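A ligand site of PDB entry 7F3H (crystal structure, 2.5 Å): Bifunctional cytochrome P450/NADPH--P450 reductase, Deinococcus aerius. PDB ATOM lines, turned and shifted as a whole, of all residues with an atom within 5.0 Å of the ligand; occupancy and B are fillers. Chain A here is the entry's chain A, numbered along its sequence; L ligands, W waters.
Water W1 lies within hydrogen-bond range of O1 of the ligand (2.5 Å) and ND1 of His 104 (2.6 Å).
Water W4 lies within hydrogen-bond range of an oxygen (O4) of the ligand and the side-chain hydroxyl of Tyr 79.
Water W2 bridges an oxygen (O4) of the ligand (2.8 Å) and the backbone carbonyl oxygen of Arg 403 (2.8 Å).
A nitrogen (N2) of the ligand lies close to the backbone carbonyl oxygen of Ala 267, at 3.3 Å.
CE1 of Phe 91 touches C33 of the ligand (3.7 Å).
Ile 156 touches the ligand.
Thr 263 touches the ligand (CG2 to C9, 3.9 Å).
Gly 268 touches the ligand (CA to C15, 3.5 Å).
Thr 271 touches the ligand (OG1 to C20, 3.2 Å).
Thr 272 touches the ligand (OG1 to C18, 3.5 Å).
CD2 of Leu 326 touches C26 of the ligand (3.2 Å).
OG1 of Thr 331 touches C26 of the ligand, 3.4 Å away.
CD1 of Ile 332 touches C27 of the ligand (3.7 Å).
Tyr 335 touches the ligand (CD1 to O4, 3.6 Å).
Pro 397 touches the ligand (O to C25, 3.3 Å).
CE1 of Phe 398 touches C22 of the ligand, 3.6 Å away.
Gly 399 touches the ligand.
O of Ala 404 touches C11 of the ligand (3.4 Å).
CG2 of Ile 406 touches C9 of the ligand, 3.5 Å away.
Gly 407 touches the ligand (CA to C14, 3.5 Å).
Phe 410 touches the ligand (CD1 to C19, 3.4 Å).
Ala 411 touches the ligand.
Hydrophobic or aromatic side chains that line the ligand: Tyr 79, Leu 90, Phe 91, Trp 100, Ile 156, Ala 267, Leu 326, Ile 332, Tyr 335, Phe 398, Ile 406, Phe 410 and Ala 411.
Of the 33 residues printed, 25 come within 4 Å of the ligand.
O3 of the ligand is in salt-bridge range of NZ of Lys 73, at 3.2 Å.
An oxygen (O2) of the ligand lies within salt-bridge range of the guanidinium group (NE) of Arg 403 (2.7 Å).
An iron atom (FE1) of the ligand is bound by the side-chain sulfur of Cys 405 (2.4 Å).
The side-chain hydroxyl of Tyr 79 lies within hydrogen-bond range of an oxygen (O3) of the ligand, at 2.5 Å.
NE1 of Trp 100 sits at hydrogen-bond distance from O1 of the ligand.
O of Leu 90 sits close to O2 of the ligand (3.0 Å).
The side-chain hydroxyl (OG1) of Thr 272 lies within hydrogen-bond range of the backbone carbonyl oxygen (O) of Gly 268 (2.7 Å).
The side-chain amino group of Lys 73 lies within hydrogen-bond range of the backbone carbonyl oxygen of Phe 91 (2.8 Å).
The side-chain hydroxyl (OG1) of Thr 331 is in hydrogen-bond range of the backbone carbonyl oxygen (O) of Thr 271 (3.1 Å).
O of Ala 267 is in hydrogen-bond range of OG1 of Thr 271.
The side-chain hydroxyl (OG1) of Thr 271 sits at hydrogen-bond distance from the backbone carbonyl oxygen (O) of Gly 268.
The backbone carbonyl oxygen (O) of Phe 398 sits at hydrogen-bond distance from the backbone NH (N) of Cys 405 (2.9 Å).
The guanidinium group (NH2) of Arg 403 lies within hydrogen-bond range of the backbone carbonyl oxygen (O) of Leu 90 (2.9 Å).
SG of Cys 405 lies close to N of Gly 407 (3.3 Å).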
ATOM      1  N   LYS A  73     -10.543  20.186  15.933  1.00  0.00           N
ATOM      2  CA  LYS A  73     -11.661  19.915  15.042  1.00  0.00           C
ATOM      3  C   LYS A  73     -12.953  20.444  15.656  1.00  0.00           C
ATOM      4  O   LYS A  73     -13.260  20.225  16.828  1.00  0.00           O
ATOM      5  CB  LYS A  73     -11.823  18.432  14.772  1.00  0.00           C
ATOM      6  CG  LYS A  73     -13.130  18.123  14.036  1.00  0.00           C
ATOM      7  CD  LYS A  73     -13.197  16.679  13.614  1.00  0.00           C
ATOM      8  CE  LYS A  73     -14.629  16.231  13.257  1.00  0.00           C
ATOM      9  NZ  LYS A  73     -14.586  14.895  12.608  1.00  0.00           N
ATOM     10  N   TYR A  79     -18.824  20.592   9.382  1.00  0.00           N
ATOM     11  CA  TYR A  79     -19.414  19.259   9.431  1.00  0.00           C
ATOM     12  C   TYR A  79     -20.922  19.293   9.674  1.00  0.00           C
ATOM     13  O   TYR A  79     -21.509  18.251   9.973  1.00  0.00           O
ATOM     14  CB  TYR A  79     -18.740  18.453  10.559  1.00  0.00           C
ATOM     15  CG  TYR A  79     -17.228  18.311  10.446  1.00  0.00           C
ATOM     16  CD1 TYR A  79     -16.363  19.317  10.898  1.00  0.00           C
ATOM     17  CD2 TYR A  79     -16.677  17.144   9.934  1.00  0.00           C
ATOM     18  CE1 TYR A  79     -14.992  19.173  10.809  1.00  0.00           C
ATOM     19  CE2 TYR A  79     -15.328  16.990   9.845  1.00  0.00           C
ATOM     20  CZ  TYR A  79     -14.481  17.995  10.287  1.00  0.00           C
ATOM     21  OH  TYR A  79     -13.125  17.761  10.159  1.00  0.00           O
ATOM     22  N   LEU A  90     -19.353   9.688  16.387  1.00  0.00           N
ATOM     23  CA  LEU A  90     -17.962  10.099  16.599  1.00  0.00           C
ATOM     24  C   LEU A  90     -17.461  11.091  15.551  1.00  0.00           C
ATOM     25  O   LEU A  90     -16.597  11.916  15.850  1.00  0.00           O
ATOM     26  CB  LEU A  90     -17.059   8.878  16.590  1.00  0.00           C
ATOM     27  CG  LEU A  90     -17.174   8.041  17.847  1.00  0.00           C
ATOM     28  CD1 LEU A  90     -16.265   6.833  17.744  1.00  0.00           C
ATOM     29  CD2 LEU A  90     -16.842   8.910  19.025  1.00  0.00           C
ATOM     30  N   PHE A  91     -17.976  11.007  14.307  1.00  0.00           N
ATOM     31  CA  PHE A  91     -17.376  11.800  13.240  1.00  0.00           C
ATOM     32  C   PHE A  91     -17.937  13.207  13.249  1.00  0.00           C
ATOM     33  O   PHE A  91     -17.228  14.168  12.910  1.00  0.00           O
ATOM     34  CB  PHE A  91     -17.614  11.150  11.885  1.00  0.00           C
ATOM     35  CG  PHE A  91     -16.902  11.811  10.723  1.00  0.00           C
ATOM     36  CD1 PHE A  91     -15.571  11.525  10.425  1.00  0.00           C
ATOM     37  CD2 PHE A  91     -17.590  12.693   9.889  1.00  0.00           C
ATOM     38  CE1 PHE A  91     -14.935  12.128   9.324  1.00  0.00           C
ATOM     39  CE2 PHE A  91     -16.959  13.298   8.796  1.00  0.00           C
ATOM     40  CZ  PHE A  91     -15.629  13.017   8.520  1.00  0.00           C
ATOM     41  N   TRP A 100     -19.670  12.038  22.605  1.00  0.00           N
ATOM     42  CA  TRP A 100     -18.395  11.804  21.934  1.00  0.00           C
ATOM     43  C   TRP A 100     -17.464  11.021  22.833  1.00  0.00           C
ATOM     44  O   TRP A 100     -17.008   9.926  22.474  1.00  0.00           O
ATOM     45  CB  TRP A 100     -17.720  13.110  21.481  1.00  0.00           C
ATOM     46  CG  TRP A 100     -16.422  12.731  20.793  1.00  0.00           C
ATOM     47  CD1 TRP A 100     -16.263  12.377  19.484  1.00  0.00           C
ATOM     48  CD2 TRP A 100     -15.114  12.587  21.397  1.00  0.00           C
ATOM     49  NE1 TRP A 100     -14.953  12.059  19.227  1.00  0.00           N
ATOM     50  CE2 TRP A 100     -14.225  12.183  20.377  1.00  0.00           C
ATOM     51  CE3 TRP A 100     -14.615  12.774  22.694  1.00  0.00           C
ATOM     52  CZ2 TRP A 100     -12.853  11.959  20.623  1.00  0.00           C
ATOM     53  CZ3 TRP A 100     -13.247  12.557  22.924  1.00  0.00           C
ATOM     54  CH2 TRP A 100     -12.384  12.161  21.887  1.00  0.00           C
ATOM     55  N   HIS A 104     -16.315   7.230  22.177  1.00  0.00           N
ATOM     56  CA  HIS A 104     -14.878   7.073  21.976  1.00  0.00           C
ATOM     57  C   HIS A 104     -14.319   6.020  22.921  1.00  0.00           C
ATOM     58  O   HIS A 104     -13.692   5.040  22.487  1.00  0.00           O
ATOM     59  CB  HIS A 104     -14.201   8.441  22.172  1.00  0.00           C
ATOM     60  CG  HIS A 104     -12.698   8.406  22.080  1.00  0.00           C
ATOM     61  ND1 HIS A 104     -12.032   8.059  20.916  1.00  0.00           N
ATOM     62  CD2 HIS A 104     -11.749   8.646  23.007  1.00  0.00           C
ATOM     63  CE1 HIS A 104     -10.729   8.098  21.139  1.00  0.00           C
ATOM     64  NE2 HIS A 104     -10.531   8.444  22.390  1.00  0.00           N
ATOM     65  N   PHE A 111     -11.812  -1.373  18.133  1.00  0.00           N
ATOM     66  CA  PHE A 111     -11.171  -0.973  16.875  1.00  0.00           C
ATOM     67  C   PHE A 111      -9.652  -1.103  16.930  1.00  0.00           C
ATOM     68  O   PHE A 111      -8.943  -0.641  16.006  1.00  0.00           O
ATOM     69  CB  PHE A 111     -11.546   0.463  16.517  1.00  0.00           C
ATOM     70  CG  PHE A 111     -12.913   0.608  15.913  1.00  0.00           C
ATOM     71  CD1 PHE A 111     -13.924   1.241  16.625  1.00  0.00           C
ATOM     72  CD2 PHE A 111     -13.172   0.163  14.622  1.00  0.00           C
ATOM     73  CE1 PHE A 111     -15.195   1.395  16.076  1.00  0.00           C
ATOM     74  CE2 PHE A 111     -14.442   0.313  14.051  1.00  0.00           C
ATOM     75  CZ  PHE A 111     -15.458   0.928  14.775  1.00  0.00           C
ATOM     76  N   ILE A 156     -18.190  -3.304   6.126  1.00  0.00           N
ATOM     77  CA  ILE A 156     -18.486  -2.514   7.301  1.00  0.00           C
ATOM     78  C   ILE A 156     -19.901  -2.831   7.800  1.00  0.00           C
ATOM     79  O   ILE A 156     -20.120  -2.861   9.010  1.00  0.00           O
ATOM     80  CB  ILE A 156     -18.221  -1.014   7.026  1.00  0.00           C
ATOM     81  CG1 ILE A 156     -18.024  -0.269   8.338  1.00  0.00           C
ATOM     82  CG2 ILE A 156     -19.369  -0.369   6.345  1.00  0.00           C
ATOM     83  CD1 ILE A 156     -16.944  -0.883   9.232  1.00  0.00           C
ATOM     84  N   THR A 263     -22.471   6.281  11.177  1.00  0.00           N
ATOM     85  CA  THR A 263     -21.137   6.875  11.117  1.00  0.00           C
ATOM     86  C   THR A 263     -20.130   5.915  10.504  1.00  0.00           C
ATOM     87  O   THR A 263     -19.331   6.295   9.638  1.00  0.00           O
ATOM     88  CB  THR A 263     -20.726   7.303  12.549  1.00  0.00           C
ATOM     89  OG1 THR A 263     -21.661   8.269  13.038  1.00  0.00           O
ATOM     90  CG2 THR A 263     -19.349   7.926  12.591  1.00  0.00           C
ATOM     91  N   PHE A 264     -20.107   4.662  10.983  1.00  0.00           N
ATOM     92  CA  PHE A 264     -19.292   3.620  10.354  1.00  0.00           C
ATOM     93  C   PHE A 264     -19.475   3.621   8.841  1.00  0.00           C
ATOM     94  O   PHE A 264     -18.490   3.530   8.087  1.00  0.00           O
ATOM     95  CB  PHE A 264     -19.602   2.226  10.911  1.00  0.00           C
ATOM     96  CG  PHE A 264     -19.458   2.117  12.388  1.00  0.00           C
ATOM     97  CD1 PHE A 264     -18.692   3.033  13.106  1.00  0.00           C
ATOM     98  CD2 PHE A 264     -20.110   1.120  13.075  1.00  0.00           C
ATOM     99  CE1 PHE A 264     -18.586   2.947  14.484  1.00  0.00           C
ATOM    100  CE2 PHE A 264     -20.021   1.023  14.445  1.00  0.00           C
ATOM    101  CZ  PHE A 264     -19.242   1.938  15.160  1.00  0.00           C
ATOM    102  N   ALA A 267     -18.132   7.218   7.225  1.00  0.00           N
ATOM    103  CA  ALA A 267     -16.704   7.428   7.345  1.00  0.00           C
ATOM    104  C   ALA A 267     -15.905   6.223   6.870  1.00  0.00           C
ATOM    105  O   ALA A 267     -14.680   6.333   6.714  1.00  0.00           O
ATOM    106  CB  ALA A 267     -16.342   7.732   8.821  1.00  0.00           C
ATOM    107  N   GLY A 268     -16.556   5.090   6.630  1.00  0.00           N
ATOM    108  CA  GLY A 268     -15.767   3.924   6.307  1.00  0.00           C
ATOM    109  C   GLY A 268     -15.800   3.507   4.861  1.00  0.00           C
ATOM    110  O   GLY A 268     -14.852   2.845   4.423  1.00  0.00           O
ATOM    111  N   THR A 271     -13.731   6.305   2.008  1.00  0.00           N
ATOM    112  CA  THR A 271     -12.305   6.394   2.351  1.00  0.00           C
ATOM    113  C   THR A 271     -11.584   5.105   1.965  1.00  0.00           C
ATOM    114  O   THR A 271     -10.578   5.145   1.255  1.00  0.00           O
ATOM    115  CB  THR A 271     -12.137   6.646   3.852  1.00  0.00           C
ATOM    116  OG1 THR A 271     -12.994   5.765   4.595  1.00  0.00           O
ATOM    117  CG2 THR A 271     -12.433   8.072   4.203  1.00  0.00           C
ATOM    118  N   THR A 272     -12.084   3.961   2.430  1.00  0.00           N
ATOM    119  CA  THR A 272     -11.445   2.675   2.207  1.00  0.00           C
ATOM    120  C   THR A 272     -11.518   2.246   0.751  1.00  0.00           C
ATOM    121  O   THR A 272     -10.530   1.785   0.191  1.00  0.00           O
ATOM    122  CB  THR A 272     -12.108   1.659   3.116  1.00  0.00           C
ATOM    123  OG1 THR A 272     -12.171   2.255   4.421  1.00  0.00           O
ATOM    124  CG2 THR A 272     -11.333   0.356   3.142  1.00  0.00           C
ATOM    125  N   LEU A 275      -9.020   4.318  -1.064  1.00  0.00           N
ATOM    126  CA  LEU A 275      -7.656   3.821  -0.862  1.00  0.00           C
ATOM    127  C   LEU A 275      -7.401   2.633  -1.782  1.00  0.00           C
ATOM    128  O   LEU A 275      -6.330   2.546  -2.404  1.00  0.00           O
ATOM    129  CB  LEU A 275      -7.427   3.456   0.609  1.00  0.00           C
ATOM    130  CG  LEU A 275      -6.149   2.657   0.927  1.00  0.00           C
ATOM    131  CD1 LEU A 275      -4.919   3.284   0.279  1.00  0.00           C
ATOM    132  CD2 LEU A 275      -5.896   2.454   2.451  1.00  0.00           C
ATOM    133  N   LEU A 326      -1.441   5.910   0.456  1.00  0.00           N
ATOM    134  CA  LEU A 326      -2.039   6.962   1.270  1.00  0.00           C
ATOM    135  C   LEU A 326      -1.163   8.213   1.301  1.00  0.00           C
ATOM    136  O   LEU A 326      -1.658   9.310   1.506  1.00  0.00           O
ATOM    137  CB  LEU A 326      -2.296   6.432   2.687  1.00  0.00           C
ATOM    138  CG  LEU A 326      -3.482   5.488   2.906  1.00  0.00           C
ATOM    139  CD1 LEU A 326      -3.588   5.042   4.348  1.00  0.00           C
ATOM    140  CD2 LEU A 326      -4.821   6.071   2.466  1.00  0.00           C
ATOM    141  N   SER A 330      -4.201  10.199  -0.229  1.00  0.00           N
ATOM    142  CA  SER A 330      -5.020  10.170   0.979  1.00  0.00           C
ATOM    143  C   SER A 330      -6.450  10.651   0.694  1.00  0.00           C
ATOM    144  O   SER A 330      -6.655  11.757   0.173  1.00  0.00           O
ATOM    145  CB  SER A 330      -4.326  11.048   2.028  1.00  0.00           C
ATOM    146  OG  SER A 330      -4.846  10.887   3.321  1.00  0.00           O
ATOM    147  N   THR A 331      -7.430   9.823   1.059  1.00  0.00           N
ATOM    148  CA  THR A 331      -8.764   9.999   0.515  1.00  0.00           C
ATOM    149  C   THR A 331      -9.614  11.024   1.268  1.00  0.00           C
ATOM    150  O   THR A 331     -10.623  11.488   0.717  1.00  0.00           O
ATOM    151  CB  THR A 331      -9.502   8.651   0.420  1.00  0.00           C
ATOM    152  OG1 THR A 331      -9.550   8.012   1.712  1.00  0.00           O
ATOM    153  CG2 THR A 331      -8.771   7.717  -0.563  1.00  0.00           C
ATOM    154  N   ILE A 332      -9.252  11.403   2.492  1.00  0.00           N
ATOM    155  CA  ILE A 332      -9.822  12.645   3.025  1.00  0.00           C
ATOM    156  C   ILE A 332      -8.716  13.681   3.012  1.00  0.00           C
ATOM    157  O   ILE A 332      -7.894  13.732   3.949  1.00  0.00           O
ATOM    158  CB  ILE A 332     -10.435  12.518   4.433  1.00  0.00           C
ATOM    159  CG1 ILE A 332     -11.526  11.453   4.508  1.00  0.00           C
ATOM    160  CG2 ILE A 332     -11.024  13.872   4.802  1.00  0.00           C
ATOM    161  CD1 ILE A 332     -12.107  11.230   5.955  1.00  0.00           C
ATOM    162  N   TYR A 335      -9.139  18.054   5.514  1.00  0.00           N
ATOM    163  CA  TYR A 335      -9.791  18.270   6.795  1.00  0.00           C
ATOM    164  C   TYR A 335      -9.086  19.371   7.569  1.00  0.00           C
ATOM    165  O   TYR A 335      -7.880  19.618   7.385  1.00  0.00           O
ATOM    166  CB  TYR A 335      -9.834  16.977   7.596  1.00  0.00           C
ATOM    167  CG  TYR A 335      -8.494  16.380   8.016  1.00  0.00           C
ATOM    168  CD1 TYR A 335      -7.896  16.746   9.193  1.00  0.00           C
ATOM    169  CD2 TYR A 335      -7.856  15.412   7.220  1.00  0.00           C
ATOM    170  CE1 TYR A 335      -6.689  16.179   9.598  1.00  0.00           C
ATOM    171  CE2 TYR A 335      -6.641  14.827   7.634  1.00  0.00           C
ATOM    172  CZ  TYR A 335      -6.061  15.234   8.816  1.00  0.00           C
ATOM    173  OH  TYR A 335      -4.862  14.697   9.270  1.00  0.00           O
ATOM    174  N   LYS A 396      -0.411  12.429   7.741  1.00  0.00           N
ATOM    175  CA  LYS A 396      -1.649  12.507   8.514  1.00  0.00           C
ATOM    176  C   LYS A 396      -2.867  11.969   7.758  1.00  0.00           C
ATOM    177  O   LYS A 396      -3.930  12.580   7.760  1.00  0.00           O
ATOM    178  CB  LYS A 396      -1.881  13.971   8.907  1.00  0.00           C
ATOM    179  CG  LYS A 396      -0.836  14.579   9.852  1.00  0.00           C
ATOM    180  CD  LYS A 396      -0.690  13.755  11.097  1.00  0.00           C
ATOM    181  CE  LYS A 396      -0.408  14.616  12.282  1.00  0.00           C
ATOM    182  NZ  LYS A 396      -0.516  13.802  13.503  1.00  0.00           N
ATOM    183  N   PRO A 397      -2.762  10.770   7.141  1.00  0.00           N
ATOM    184  CA  PRO A 397      -3.911  10.277   6.359  1.00  0.00           C
ATOM    185  C   PRO A 397      -5.069   9.824   7.238  1.00  0.00           C
ATOM    186  O   PRO A 397      -6.199   9.711   6.744  1.00  0.00           O
ATOM    187  CB  PRO A 397      -3.332   9.115   5.556  1.00  0.00           C
ATOM    188  CG  PRO A 397      -2.233   8.610   6.380  1.00  0.00           C
ATOM    189  CD  PRO A 397      -1.690   9.768   7.224  1.00  0.00           C
ATOM    190  N   PHE A 398      -4.809   9.521   8.504  1.00  0.00           N
ATOM    191  CA  PHE A 398      -5.841   9.098   9.440  1.00  0.00           C
ATOM    192  C   PHE A 398      -6.096  10.189  10.496  1.00  0.00           C
ATOM    193  O   PHE A 398      -6.323   9.886  11.662  1.00  0.00           O
ATOM    194  CB  PHE A 398      -5.488   7.744  10.064  1.00  0.00           C
ATOM    195  CG  PHE A 398      -5.478   6.605   9.060  1.00  0.00           C
ATOM    196  CD1 PHE A 398      -6.676   6.083   8.549  1.00  0.00           C
ATOM    197  CD2 PHE A 398      -4.276   6.084   8.580  1.00  0.00           C
ATOM    198  CE1 PHE A 398      -6.676   5.042   7.626  1.00  0.00           C
ATOM    199  CE2 PHE A 398      -4.261   5.038   7.632  1.00  0.00           C
ATOM    200  CZ  PHE A 398      -5.462   4.514   7.167  1.00  0.00           C
ATOM    201  N   GLY A 399      -5.999  11.463  10.085  1.00  0.00           N
ATOM    202  CA  GLY A 399      -6.337  12.557  10.985  1.00  0.00           C
ATOM    203  C   GLY A 399      -5.310  12.757  12.085  1.00  0.00           C
ATOM    204  O   GLY A 399      -4.151  12.334  12.008  1.00  0.00           O
ATOM    205  N   MET A 402      -6.864  13.182  19.350  1.00  0.00           N
ATOM    206  CA  MET A 402      -8.064  12.479  19.818  1.00  0.00           C
ATOM    207  C   MET A 402      -9.081  12.295  18.698  1.00  0.00           C
ATOM    208  O   MET A 402      -9.851  11.327  18.720  1.00  0.00           O
ATOM    209  CB  MET A 402      -8.718  13.251  20.974  1.00  0.00           C
ATOM    210  CG  MET A 402      -7.976  13.226  22.304  1.00  0.00           C
ATOM    211  SD  MET A 402      -7.538  11.570  22.850  1.00  0.00           S
ATOM    212  CE  MET A 402      -5.823  11.838  23.306  1.00  0.00           C
ATOM    213  N   ARG A 403      -9.101  13.210  17.723  1.00  0.00           N
ATOM    214  CA  ARG A 403     -10.004  13.163  16.583  1.00  0.00           C
ATOM    215  C   ARG A 403      -9.402  12.386  15.397  1.00  0.00           C
ATOM    216  O   ARG A 403      -9.764  12.620  14.239  1.00  0.00           O
ATOM    217  CB  ARG A 403     -10.390  14.581  16.186  1.00  0.00           C
ATOM    218  CG  ARG A 403     -11.058  15.295  17.357  1.00  0.00           C
ATOM    219  CD  ARG A 403     -12.167  14.439  17.993  1.00  0.00           C
ATOM    220  NE  ARG A 403     -13.282  14.170  17.055  1.00  0.00           N
ATOM    221  CZ  ARG A 403     -14.426  14.854  17.006  1.00  0.00           C
ATOM    222  NH1 ARG A 403     -14.672  15.852  17.839  1.00  0.00           N
ATOM    223  NH2 ARG A 403     -15.352  14.532  16.132  1.00  0.00           N
ATOM    224  N   ALA A 404      -8.466  11.482  15.663  1.00  0.00           N
ATOM    225  CA  ALA A 404      -7.914  10.660  14.610  1.00  0.00           C
ATOM    226  C   ALA A 404      -8.916   9.575  14.210  1.00  0.00           C
ATOM    227  O   ALA A 404      -9.930   9.336  14.885  1.00  0.00           O
ATOM    228  CB  ALA A 404      -6.603  10.040  15.064  1.00  0.00           C
ATOM    229  N   CYS A 405      -8.661   8.954  13.059  1.00  0.00           N
ATOM    230  CA  CYS A 405      -9.483   7.858  12.568  1.00  0.00           C
ATOM    231  C   CYS A 405      -9.552   6.717  13.572  1.00  0.00           C
ATOM    232  O   CYS A 405      -8.532   6.106  13.887  1.00  0.00           O
ATOM    233  CB  CYS A 405      -8.941   7.337  11.225  1.00  0.00           C
ATOM    234  SG  CYS A 405      -9.989   6.053  10.473  1.00  0.00           S
ATOM    235  N   ILE A 406     -10.742   6.395  14.063  1.00  0.00           N
ATOM    236  CA  ILE A 406     -10.846   5.205  14.914  1.00  0.00           C
ATOM    237  C   ILE A 406     -10.903   3.938  14.086  1.00  0.00           C
ATOM    238  O   ILE A 406     -10.690   2.847  14.632  1.00  0.00           O
ATOM    239  CB  ILE A 406     -12.088   5.277  15.815  1.00  0.00           C
ATOM    240  CG1 ILE A 406     -11.950   4.369  17.047  1.00  0.00           C
ATOM    241  CG2 ILE A 406     -13.346   4.965  15.014  1.00  0.00           C
ATOM    242  CD1 ILE A 406     -13.047   4.668  18.083  1.00  0.00           C
ATOM    243  N   GLY A 407     -11.234   4.045  12.794  1.00  0.00           N
ATOM    244  CA  GLY A 407     -11.383   2.937  11.879  1.00  0.00           C
ATOM    245  C   GLY A 407     -10.104   2.497  11.192  1.00  0.00           C
ATOM    246  O   GLY A 407     -10.147   1.512  10.456  1.00  0.00           O
ATOM    247  N   ARG A 408      -8.967   3.152  11.486  1.00  0.00           N
ATOM    248  CA  ARG A 408      -7.720   2.939  10.759  1.00  0.00           C
ATOM    249  C   ARG A 408      -7.350   1.456  10.652  1.00  0.00           C
ATOM    250  O   ARG A 408      -7.066   0.956   9.552  1.00  0.00           O
ATOM    251  CB  ARG A 408      -6.577   3.691  11.450  1.00  0.00           C
ATOM    252  CG  ARG A 408      -5.214   3.423  10.873  1.00  0.00           C
ATOM    253  CD  ARG A 408      -4.049   4.146  11.631  1.00  0.00           C
ATOM    254  NE  ARG A 408      -2.773   3.638  11.121  1.00  0.00           N
ATOM    255  CZ  ARG A 408      -2.240   2.465  11.485  1.00  0.00           C
ATOM    256  NH1 ARG A 408      -2.876   1.718  12.367  1.00  0.00           N
ATOM    257  NH2 ARG A 408      -1.084   2.030  10.972  1.00  0.00           N
ATOM    258  N   PHE A 410      -9.173  -1.273  11.112  1.00  0.00           N
ATOM    259  CA  PHE A 410     -10.168  -1.959  10.294  1.00  0.00           C
ATOM    260  C   PHE A 410      -9.917  -1.717   8.813  1.00  0.00           C
ATOM    261  O   PHE A 410      -9.865  -2.655   8.006  1.00  0.00           O
ATOM    262  CB  PHE A 410     -11.571  -1.501  10.691  1.00  0.00           C
ATOM    263  CG  PHE A 410     -12.681  -2.385  10.164  1.00  0.00           C
ATOM    264  CD1 PHE A 410     -13.155  -2.215   8.869  1.00  0.00           C
ATOM    265  CD2 PHE A 410     -13.247  -3.369  10.982  1.00  0.00           C
ATOM    266  CE1 PHE A 410     -14.178  -3.008   8.398  1.00  0.00           C
ATOM    267  CE2 PHE A 410     -14.266  -4.159  10.525  1.00  0.00           C
ATOM    268  CZ  PHE A 410     -14.741  -3.990   9.230  1.00  0.00           C
ATOM    269  N   ALA A 411      -9.750  -0.446   8.443  1.00  0.00           N
ATOM    270  CA  ALA A 411      -9.539  -0.107   7.037  1.00  0.00           C
ATOM    271  C   ALA A 411      -8.333  -0.836   6.483  1.00  0.00           C
ATOM    272  O   ALA A 411      -8.461  -1.581   5.495  1.00  0.00           O
ATOM    273  CB  ALA A 411      -9.354   1.411   6.899  1.00  0.00           C
HETATM  274  C1  LIG L   1     -12.048   9.885  11.358  1.00  0.00           C
HETATM  275  C2  LIG L   1     -14.289   5.575  11.063  1.00  0.00           C
HETATM  276  C3  LIG L   1     -11.520   4.424   7.214  1.00  0.00           C
HETATM  277  C4  LIG L   1      -9.506   8.839   7.342  1.00  0.00           C
HETATM  278  C5  LIG L   1     -12.883   8.819  11.609  1.00  0.00           C
HETATM  279  C6  LIG L   1     -13.905   8.777  12.628  1.00  0.00           C
HETATM  280  C7  LIG L   1     -14.515   7.580  12.590  1.00  0.00           C
HETATM  281  C8  LIG L   1     -13.936   6.848  11.476  1.00  0.00           C
HETATM  282  C9  LIG L   1     -15.663   7.106  13.515  1.00  0.00           C
HETATM  283  C10 LIG L   1     -14.144   9.903  13.652  1.00  0.00           C
HETATM  284  C11 LIG L   1     -13.299   9.574  14.891  1.00  0.00           C
HETATM  285  C12 LIG L   1     -13.519  10.587  16.020  1.00  0.00           C
HETATM  286  O1  LIG L   1     -13.701  10.108  17.177  1.00  0.00           O
HETATM  287  O2  LIG L   1     -13.610  11.833  15.821  1.00  0.00           O
HETATM  288  C13 LIG L   1     -13.719   4.857  10.024  1.00  0.00           C
HETATM  289  C14 LIG L   1     -14.034   3.497   9.639  1.00  0.00           C
HETATM  290  C15 LIG L   1     -13.229   3.174   8.612  1.00  0.00           C
HETATM  291  C16 LIG L   1     -12.433   4.346   8.270  1.00  0.00           C
HETATM  292  C17 LIG L   1     -15.056   2.597  10.371  1.00  0.00           C
HETATM  293  C18 LIG L   1     -13.153   1.896   7.735  1.00  0.00           C
HETATM  294  C19 LIG L   1     -14.016   0.877   7.806  1.00  0.00           C
HETATM  295  C20 LIG L   1     -10.731   5.519   6.895  1.00  0.00           C
HETATM  296  C21 LIG L   1      -9.715   5.604   5.840  1.00  0.00           C
HETATM  297  C22 LIG L   1      -9.210   6.851   5.912  1.00  0.00           C
HETATM  298  C23 LIG L   1      -9.828   7.547   6.998  1.00  0.00           C
HETATM  299  C24 LIG L   1      -9.365   4.468   4.826  1.00  0.00           C
HETATM  300  C25 LIG L   1      -8.126   7.552   5.104  1.00  0.00           C
HETATM  301  C26 LIG L   1      -7.457   6.938   4.138  1.00  0.00           C
HETATM  302  C27 LIG L   1     -10.017   9.503   8.428  1.00  0.00           C
HETATM  303  C28 LIG L   1      -9.715  10.884   8.812  1.00  0.00           C
HETATM  304  C29 LIG L   1     -10.417  11.147   9.912  1.00  0.00           C
HETATM  305  C30 LIG L   1     -11.201   9.978  10.272  1.00  0.00           C
HETATM  306  C31 LIG L   1      -8.748  11.871   8.101  1.00  0.00           C
HETATM  307  C32 LIG L   1     -10.403  12.468  10.645  1.00  0.00           C
HETATM  308  C33 LIG L   1     -11.472  13.270   9.944  1.00  0.00           C
HETATM  309  C34 LIG L   1     -11.505  14.679  10.443  1.00  0.00           C
HETATM  310  O3  LIG L   1     -12.570  15.296  10.206  1.00  0.00           O
HETATM  311  O4  LIG L   1     -10.502  15.164  11.058  1.00  0.00           O
HETATM  312  N1  LIG L   1     -12.961   7.628  10.906  1.00  0.00           N
HETATM  313  N2  LIG L   1     -12.737   5.341   9.187  1.00  0.00           N
HETATM  314  N3  LIG L   1     -10.776   6.737   7.567  1.00  0.00           N
HETATM  315  N4  LIG L   1     -10.927   8.993   9.347  1.00  0.00           N
HETATM  316 FE1  LIG L   1     -11.735   7.182   9.327  1.00  0.00          FE
HETATM  317  O   HOH W   1     -12.725   8.118  18.428  1.00  0.00           O
HETATM  318  O   HOH W   2      -8.420  14.718  12.878  1.00  0.00           O
HETATM  319  O   HOH W   3     -13.175  15.557   7.293  1.00  0.00           O
HETATM  320  O   HOH W   4     -10.416  17.767  11.847  1.00  0.00           O
